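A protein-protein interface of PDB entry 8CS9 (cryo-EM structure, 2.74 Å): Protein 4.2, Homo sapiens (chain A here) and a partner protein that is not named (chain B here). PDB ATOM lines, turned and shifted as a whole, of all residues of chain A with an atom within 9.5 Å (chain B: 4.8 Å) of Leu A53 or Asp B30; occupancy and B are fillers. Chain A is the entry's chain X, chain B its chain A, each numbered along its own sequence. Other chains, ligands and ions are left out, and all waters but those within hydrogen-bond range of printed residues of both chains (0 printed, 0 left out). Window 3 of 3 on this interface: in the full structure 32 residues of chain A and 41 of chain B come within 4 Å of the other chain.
Leu A53 touches just these residues of chain B: Asp B26 (3.8 Å), Lys B27 (3.8 Å) and Asp B30 (3.5 Å). Ala A55 touches none of the printed residues of chain B. Printed residues of chain B within 4 Å of Ser A83: Asp B26 and Leu B29. Of the printed residues of chain B, Arg A97 touches Asp B30 (2.3 Å) and Arg B33 (3.0 Å). Printed residues of chain A within 4 Å of Leu B29: Ser A83 (3.3 Å). Asp B30 touches two residues of chain A. The nearest printed residue of chain B that does not touch Leu A53 is His B31 (6.1 Å). The nearest printed residue of chain A that does not touch Asp B26 is Ile A81 (4.4 Å).
Leu A53 touches Asp B26 (CD2 to C, 3.8 Å). Leu A53 touches Lys B27 (CD2 to N, 3.8 Å). Leu A53 touches Asp B30. Leu A56 touches Asp B26 (CD2 to OD2, 3.7 Å). CB of Ser A82 touches OD2 of Asp B26, at 3.3 Å. Leu B29 touches Ser A83.
Of the 18 printed residues of chain A, 5 touch a printed residue of chain B. Printed residues of chain A that touch a printed residue of chain B: Leu A53, Leu A56, Ser A82, Ser A83 and Arg A97. Hydrophobic or aromatic side chains of chain A that line the printed part of chain B: Leu A53 and Leu A56. Of the 9 printed residues of chain B, 5 touch a printed residue of chain A. Hydrophobic or aromatic side chains of chain B within 4 Å of the printed part of chain A: Leu B29. Among the printed residues, Asp or Glu carboxylates within 4 Å of a Lys or Arg side-chain nitrogen of the other chain: Arg A97 with Asp B30.
N of Ser A83 lies within hydrogen-bond range of OD1 of Asp B26. OD1 of Asp B30 lies within salt-bridge range of NH1 of Arg A97 (3.3 Å). The guanidinium group of Arg B33 is in hydrogen-bond range of the backbone carbonyl oxygen of Arg A97.
The side-chain amide nitrogen (ND2) of Asn B34 lies close to the backbone carbonyl oxygen (O) of Asp B30 (3.1 Å).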
ATOM      1  N   LEU A   5      12.903 -17.838  24.806  1.00  0.00           N
ATOM      2  CA  LEU A   5      11.576 -17.359  25.175  1.00  0.00           C
ATOM      3  C   LEU A   5      10.824 -18.422  25.961  1.00  0.00           C
ATOM      4  O   LEU A   5       9.638 -18.671  25.729  1.00  0.00           O
ATOM      5  CB  LEU A   5      10.784 -16.939  23.942  1.00  0.00           C
ATOM      6  CG  LEU A   5      10.107 -15.570  23.995  1.00  0.00           C
ATOM      7  CD1 LEU A   5      11.060 -14.518  24.528  1.00  0.00           C
ATOM      8  CD2 LEU A   5       9.591 -15.185  22.622  1.00  0.00           C
ATOM      9  N   VAL A  49      13.910 -11.174  28.773  1.00  0.00           N
ATOM     10  CA  VAL A  49      13.714 -11.000  27.340  1.00  0.00           C
ATOM     11  C   VAL A  49      14.562  -9.821  26.883  1.00  0.00           C
ATOM     12  O   VAL A  49      14.337  -8.682  27.306  1.00  0.00           O
ATOM     13  CB  VAL A  49      12.232 -10.780  27.003  1.00  0.00           C
ATOM     14  CG1 VAL A  49      12.011 -10.880  25.509  1.00  0.00           C
ATOM     15  CG2 VAL A  49      11.369 -11.795  27.733  1.00  0.00           C
ATOM     16  N   ARG A  50      15.540 -10.094  26.018  1.00  0.00           N
ATOM     17  CA  ARG A  50      16.465  -9.053  25.584  1.00  0.00           C
ATOM     18  C   ARG A  50      15.777  -8.055  24.661  1.00  0.00           C
ATOM     19  O   ARG A  50      15.700  -6.859  24.966  1.00  0.00           O
ATOM     20  CB  ARG A  50      17.676  -9.686  24.894  1.00  0.00           C
ATOM     21  N   ALA A  51      15.267  -8.528  23.529  1.00  0.00           N
ATOM     22  CA  ALA A  51      14.603  -7.682  22.545  1.00  0.00           C
ATOM     23  C   ALA A  51      13.115  -7.995  22.553  1.00  0.00           C
ATOM     24  O   ALA A  51      12.716  -9.136  22.305  1.00  0.00           O
ATOM     25  CB  ALA A  51      15.200  -7.893  21.154  1.00  0.00           C
ATOM     26  N   PHE A  52      12.297  -6.979  22.836  1.00  0.00           N
ATOM     27  CA  PHE A  52      10.867  -7.213  23.009  1.00  0.00           C
ATOM     28  C   PHE A  52      10.159  -7.441  21.679  1.00  0.00           C
ATOM     29  O   PHE A  52       9.298  -8.319  21.581  1.00  0.00           O
ATOM     30  CB  PHE A  52      10.228  -6.043  23.750  1.00  0.00           C
ATOM     31  CG  PHE A  52       8.730  -6.111  23.800  1.00  0.00           C
ATOM     32  CD1 PHE A  52       8.094  -7.108  24.518  1.00  0.00           C
ATOM     33  CD2 PHE A  52       7.957  -5.188  23.118  1.00  0.00           C
ATOM     34  CE1 PHE A  52       6.717  -7.177  24.562  1.00  0.00           C
ATOM     35  CE2 PHE A  52       6.581  -5.251  23.164  1.00  0.00           C
ATOM     36  CZ  PHE A  52       5.961  -6.249  23.887  1.00  0.00           C
ATOM     37  N   LEU A  53      10.479  -6.642  20.654  1.00  0.00           N
ATOM     38  CA  LEU A  53       9.738  -6.733  19.394  1.00  0.00           C
ATOM     39  C   LEU A  53       9.927  -8.069  18.677  1.00  0.00           C
ATOM     40  O   LEU A  53       8.916  -8.666  18.259  1.00  0.00           O
ATOM     41  CB  LEU A  53      10.088  -5.539  18.500  1.00  0.00           C
ATOM     42  CG  LEU A  53       9.593  -4.178  18.997  1.00  0.00           C
ATOM     43  CD1 LEU A  53      10.356  -3.040  18.337  1.00  0.00           C
ATOM     44  CD2 LEU A  53       8.101  -4.029  18.762  1.00  0.00           C
ATOM     45  N   PRO A  54      11.151  -8.591  18.478  1.00  0.00           N
ATOM     46  CA  PRO A  54      11.257  -9.930  17.868  1.00  0.00           C
ATOM     47  C   PRO A  54      10.601 -11.017  18.698  1.00  0.00           C
ATOM     48  O   PRO A  54      10.045 -11.970  18.138  1.00  0.00           O
ATOM     49  CB  PRO A  54      12.773 -10.145  17.742  1.00  0.00           C
ATOM     50  CG  PRO A  54      13.367  -8.800  17.823  1.00  0.00           C
ATOM     51  CD  PRO A  54      12.487  -8.017  18.728  1.00  0.00           C
ATOM     52  N   ALA A  55      10.655 -10.900  20.027  1.00  0.00           N
ATOM     53  CA  ALA A  55       9.962 -11.854  20.884  1.00  0.00           C
ATOM     54  C   ALA A  55       8.455 -11.780  20.679  1.00  0.00           C
ATOM     55  O   ALA A  55       7.766 -12.805  20.696  1.00  0.00           O
ATOM     56  CB  ALA A  55      10.320 -11.598  22.345  1.00  0.00           C
ATOM     57  N   LEU A  56       7.929 -10.568  20.492  1.00  0.00           N
ATOM     58  CA  LEU A  56       6.507 -10.400  20.223  1.00  0.00           C
ATOM     59  C   LEU A  56       6.126 -11.009  18.883  1.00  0.00           C
ATOM     60  O   LEU A  56       5.027 -11.554  18.732  1.00  0.00           O
ATOM     61  CB  LEU A  56       6.142  -8.917  20.259  1.00  0.00           C
ATOM     62  CG  LEU A  56       4.714  -8.582  20.684  1.00  0.00           C
ATOM     63  CD1 LEU A  56       4.360  -9.268  21.995  1.00  0.00           C
ATOM     64  CD2 LEU A  56       4.514  -7.083  20.775  1.00  0.00           C
ATOM     65  N   LYS A  57       7.018 -10.919  17.895  1.00  0.00           N
ATOM     66  CA  LYS A  57       6.750 -11.542  16.603  1.00  0.00           C
ATOM     67  C   LYS A  57       6.717 -13.063  16.679  1.00  0.00           C
ATOM     68  O   LYS A  57       6.114 -13.700  15.809  1.00  0.00           O
ATOM     69  CB  LYS A  57       7.800 -11.109  15.578  1.00  0.00           C
ATOM     70  CG  LYS A  57       7.586  -9.725  15.000  1.00  0.00           C
ATOM     71  CD  LYS A  57       8.828  -9.249  14.263  1.00  0.00           C
ATOM     72  CE  LYS A  57       9.061  -7.761  14.461  1.00  0.00           C
ATOM     73  NZ  LYS A  57      10.479  -7.465  14.811  1.00  0.00           N
ATOM     74  N   LYS A  58       7.340 -13.658  17.693  1.00  0.00           N
ATOM     75  CA  LYS A  58       7.516 -15.101  17.763  1.00  0.00           C
ATOM     76  C   LYS A  58       6.428 -15.815  18.558  1.00  0.00           C
ATOM     77  O   LYS A  58       6.446 -17.047  18.624  1.00  0.00           O
ATOM     78  CB  LYS A  58       8.882 -15.431  18.377  1.00  0.00           C
ATOM     79  CG  LYS A  58      10.056 -15.247  17.434  1.00  0.00           C
ATOM     80  CD  LYS A  58      11.323 -15.864  18.009  1.00  0.00           C
ATOM     81  CE  LYS A  58      12.455 -14.850  18.075  1.00  0.00           C
ATOM     82  NZ  LYS A  58      12.524 -14.162  19.396  1.00  0.00           N
ATOM     83  N   VAL A  59       5.482 -15.090  19.153  1.00  0.00           N
ATOM     84  CA  VAL A  59       4.519 -15.693  20.066  1.00  0.00           C
ATOM     85  C   VAL A  59       3.114 -15.536  19.497  1.00  0.00           C
ATOM     86  O   VAL A  59       2.773 -14.514  18.894  1.00  0.00           O
ATOM     87  CB  VAL A  59       4.605 -15.078  21.483  1.00  0.00           C
ATOM     88  CG1 VAL A  59       3.342 -15.324  22.247  1.00  0.00           C
ATOM     89  CG2 VAL A  59       5.777 -15.649  22.246  1.00  0.00           C
ATOM     90  N   ILE A  81      -0.081 -11.672  19.630  1.00  0.00           N
ATOM     91  CA  ILE A  81      -0.030 -10.652  20.670  1.00  0.00           C
ATOM     92  C   ILE A  81       0.505  -9.385  20.015  1.00  0.00           C
ATOM     93  O   ILE A  81       1.704  -9.263  19.762  1.00  0.00           O
ATOM     94  CB  ILE A  81       0.825 -11.088  21.863  1.00  0.00           C
ATOM     95  CG1 ILE A  81       0.496 -12.526  22.260  1.00  0.00           C
ATOM     96  CG2 ILE A  81       0.614 -10.159  23.043  1.00  0.00           C
ATOM     97  CD1 ILE A  81       1.261 -13.000  23.464  1.00  0.00           C
ATOM     98  N   SER A  82      -0.387  -8.440  19.729  1.00  0.00           N
ATOM     99  CA  SER A  82       0.005  -7.208  19.061  1.00  0.00           C
ATOM    100  C   SER A  82      -1.035  -6.135  19.335  1.00  0.00           C
ATOM    101  O   SER A  82      -2.170  -6.426  19.721  1.00  0.00           O
ATOM    102  CB  SER A  82       0.169  -7.414  17.551  1.00  0.00           C
ATOM    103  OG  SER A  82      -0.834  -8.270  17.039  1.00  0.00           O
ATOM    104  N   SER A  83      -0.627  -4.883  19.127  1.00  0.00           N
ATOM    105  CA  SER A  83      -1.553  -3.762  19.208  1.00  0.00           C
ATOM    106  C   SER A  83      -2.439  -3.646  17.976  1.00  0.00           C
ATOM    107  O   SER A  83      -3.360  -2.825  17.974  1.00  0.00           O
ATOM    108  CB  SER A  83      -0.781  -2.459  19.419  1.00  0.00           C
ATOM    109  OG  SER A  83      -0.684  -2.140  20.794  1.00  0.00           O
ATOM    110  N   VAL A  94       0.178  -6.563  24.824  1.00  0.00           N
ATOM    111  CA  VAL A  94       0.958  -6.342  26.038  1.00  0.00           C
ATOM    112  C   VAL A  94       0.718  -4.910  26.505  1.00  0.00           C
ATOM    113  O   VAL A  94       1.146  -3.954  25.855  1.00  0.00           O
ATOM    114  CB  VAL A  94       2.448  -6.609  25.801  1.00  0.00           C
ATOM    115  CG1 VAL A  94       3.266  -6.192  27.012  1.00  0.00           C
ATOM    116  CG2 VAL A  94       2.675  -8.076  25.478  1.00  0.00           C
ATOM    117  N   ARG A  97       5.059  -4.390  30.723  1.00  0.00           N
ATOM    118  CA  ARG A  97       6.091  -5.410  30.672  1.00  0.00           C
ATOM    119  C   ARG A  97       7.289  -4.968  31.493  1.00  0.00           C
ATOM    120  O   ARG A  97       7.530  -3.774  31.684  1.00  0.00           O
ATOM    121  CB  ARG A  97       6.537  -5.690  29.235  1.00  0.00           C
ATOM    122  CG  ARG A  97       6.971  -4.449  28.489  1.00  0.00           C
ATOM    123  CD  ARG A  97       7.503  -4.783  27.121  1.00  0.00           C
ATOM    124  NE  ARG A  97       7.294  -3.688  26.184  1.00  0.00           N
ATOM    125  CZ  ARG A  97       8.270  -3.017  25.592  1.00  0.00           C
ATOM    126  NH1 ARG A  97       9.541  -3.315  25.804  1.00  0.00           N
ATOM    127  NH2 ARG A  97       7.963  -2.025  24.761  1.00  0.00           N
ATOM    128  N   TRP A 102       5.283 -10.257  31.024  1.00  0.00           N
ATOM    129  CA  TRP A 102       4.396  -9.501  30.149  1.00  0.00           C
ATOM    130  C   TRP A 102       3.005  -9.470  30.766  1.00  0.00           C
ATOM    131  O   TRP A 102       2.482 -10.512  31.172  1.00  0.00           O
ATOM    132  CB  TRP A 102       4.316 -10.121  28.750  1.00  0.00           C
ATOM    133  CG  TRP A 102       5.548  -9.988  27.909  1.00  0.00           C
ATOM    134  CD1 TRP A 102       6.692  -9.316  28.219  1.00  0.00           C
ATOM    135  CD2 TRP A 102       5.755 -10.556  26.612  1.00  0.00           C
ATOM    136  NE1 TRP A 102       7.599  -9.426  27.194  1.00  0.00           N
ATOM    137  CE2 TRP A 102       7.047 -10.186  26.196  1.00  0.00           C
ATOM    138  CE3 TRP A 102       4.970 -11.340  25.761  1.00  0.00           C
ATOM    139  CZ2 TRP A 102       7.574 -10.572  24.966  1.00  0.00           C
ATOM    140  CZ3 TRP A 102       5.495 -11.724  24.543  1.00  0.00           C
ATOM    141  CH2 TRP A 102       6.783 -11.338  24.156  1.00  0.00           C
ATOM    142  N   ASP B  26       3.231  -1.566  17.220  1.00  0.00           N
ATOM    143  CA  ASP B  26       4.058  -2.103  18.295  1.00  0.00           C
ATOM    144  C   ASP B  26       5.405  -1.392  18.373  1.00  0.00           C
ATOM    145  O   ASP B  26       5.856  -1.027  19.467  1.00  0.00           O
ATOM    146  CB  ASP B  26       4.248  -3.606  18.108  1.00  0.00           C
ATOM    147  CG  ASP B  26       3.022  -4.400  18.508  1.00  0.00           C
ATOM    148  OD1 ASP B  26       2.313  -3.968  19.439  1.00  0.00           O
ATOM    149  OD2 ASP B  26       2.763  -5.453  17.890  1.00  0.00           O
ATOM    150  N   LYS B  27       6.053  -1.171  17.228  1.00  0.00           N
ATOM    151  CA  LYS B  27       7.326  -0.455  17.226  1.00  0.00           C
ATOM    152  C   LYS B  27       7.152   0.990  17.679  1.00  0.00           C
ATOM    153  O   LYS B  27       7.992   1.519  18.416  1.00  0.00           O
ATOM    154  CB  LYS B  27       7.961  -0.513  15.838  1.00  0.00           C
ATOM    155  CG  LYS B  27       9.358   0.080  15.775  1.00  0.00           C
ATOM    156  CD  LYS B  27       9.911   0.060  14.360  1.00  0.00           C
ATOM    157  CE  LYS B  27      11.343  -0.439  14.332  1.00  0.00           C
ATOM    158  NZ  LYS B  27      11.427  -1.907  14.560  1.00  0.00           N
ATOM    159  N   ALA B  28       6.074   1.647  17.243  1.00  0.00           N
ATOM    160  CA  ALA B  28       5.828   3.027  17.653  1.00  0.00           C
ATOM    161  C   ALA B  28       5.564   3.124  19.149  1.00  0.00           C
ATOM    162  O   ALA B  28       6.047   4.050  19.814  1.00  0.00           O
ATOM    163  CB  ALA B  28       4.657   3.608  16.861  1.00  0.00           C
ATOM    164  N   LEU B  29       4.801   2.177  19.697  1.00  0.00           N
ATOM    165  CA  LEU B  29       4.564   2.150  21.136  1.00  0.00           C
ATOM    166  C   LEU B  29       5.853   1.879  21.901  1.00  0.00           C
ATOM    167  O   LEU B  29       6.082   2.459  22.968  1.00  0.00           O
ATOM    168  CB  LEU B  29       3.499   1.106  21.469  1.00  0.00           C
ATOM    169  CG  LEU B  29       2.062   1.557  21.207  1.00  0.00           C
ATOM    170  CD1 LEU B  29       1.071   0.521  21.690  1.00  0.00           C
ATOM    171  CD2 LEU B  29       1.805   2.897  21.868  1.00  0.00           C
ATOM    172  N   ASP B  30       6.711   1.005  21.368  1.00  0.00           N
ATOM    173  CA  ASP B  30       8.019   0.779  21.976  1.00  0.00           C
ATOM    174  C   ASP B  30       8.847   2.059  21.994  1.00  0.00           C
ATOM    175  O   ASP B  30       9.481   2.388  23.003  1.00  0.00           O
ATOM    176  CB  ASP B  30       8.755  -0.328  21.223  1.00  0.00           C
ATOM    177  CG  ASP B  30       9.714  -1.096  22.107  1.00  0.00           C
ATOM    178  OD1 ASP B  30       9.514  -1.103  23.338  1.00  0.00           O
ATOM    179  OD2 ASP B  30      10.669  -1.694  21.570  1.00  0.00           O
ATOM    180  N   HIS B  31       8.849   2.795  20.881  1.00  0.00           N
ATOM    181  CA  HIS B  31       9.609   4.039  20.813  1.00  0.00           C
ATOM    182  C   HIS B  31       9.070   5.072  21.795  1.00  0.00           C
ATOM    183  O   HIS B  31       9.844   5.774  22.455  1.00  0.00           O
ATOM    184  CB  HIS B  31       9.591   4.589  19.389  1.00  0.00           C
ATOM    185  CG  HIS B  31      10.517   3.877  18.456  1.00  0.00           C
ATOM    186  ND1 HIS B  31      11.866   3.743  18.706  1.00  0.00           N
ATOM    187  CD2 HIS B  31      10.292   3.259  17.272  1.00  0.00           C
ATOM    188  CE1 HIS B  31      12.430   3.072  17.718  1.00  0.00           C
ATOM    189  NE2 HIS B  31      11.497   2.767  16.836  1.00  0.00           N
ATOM    190  N   LEU B  32       7.744   5.175  21.910  1.00  0.00           N
ATOM    191  CA  LEU B  32       7.162   6.104  22.874  1.00  0.00           C
ATOM    192  C   LEU B  32       7.469   5.681  24.305  1.00  0.00           C
ATOM    193  O   LEU B  32       7.612   6.531  25.191  1.00  0.00           O
ATOM    194  CB  LEU B  32       5.654   6.220  22.654  1.00  0.00           C
ATOM    195  CG  LEU B  32       5.227   6.863  21.334  1.00  0.00           C
ATOM    196  CD1 LEU B  32       3.737   6.690  21.104  1.00  0.00           C
ATOM    197  CD2 LEU B  32       5.611   8.332  21.317  1.00  0.00           C
ATOM    198  N   ARG B  33       7.557   4.373  24.554  1.00  0.00           N
ATOM    199  CA  ARG B  33       7.961   3.892  25.870  1.00  0.00           C
ATOM    200  C   ARG B  33       9.405   4.275  26.176  1.00  0.00           C
ATOM    201  O   ARG B  33       9.727   4.681  27.298  1.00  0.00           O
ATOM    202  CB  ARG B  33       7.776   2.378  25.953  1.00  0.00           C
ATOM    203  CG  ARG B  33       8.072   1.787  27.321  1.00  0.00           C
ATOM    204  CD  ARG B  33       7.336   0.473  27.515  1.00  0.00           C
ATOM    205  NE  ARG B  33       7.687  -0.180  28.770  1.00  0.00           N
ATOM    206  CZ  ARG B  33       8.734  -0.976  28.930  1.00  0.00           C
ATOM    207  NH1 ARG B  33       9.571  -1.226  27.937  1.00  0.00           N
ATOM    208  NH2 ARG B  33       8.949  -1.535  30.118  1.00  0.00           N
ATOM    209  N   ASN B  34      10.291   4.152  25.183  1.00  0.00           N
ATOM    210  CA  ASN B  34      11.703   4.451  25.405  1.00  0.00           C
ATOM    211  C   ASN B  34      11.971   5.939  25.591  1.00  0.00           C
ATOM    212  O   ASN B  34      13.062   6.303  26.039  1.00  0.00           O
ATOM    213  CB  ASN B  34      12.557   3.919  24.251  1.00  0.00           C
ATOM    214  CG  ASN B  34      12.343   2.439  23.987  1.00  0.00           C
ATOM    215  OD1 ASN B  34      11.949   1.691  24.883  1.00  0.00           O
ATOM    216  ND2 ASN B  34      12.580   2.012  22.752  1.00  0.00           N
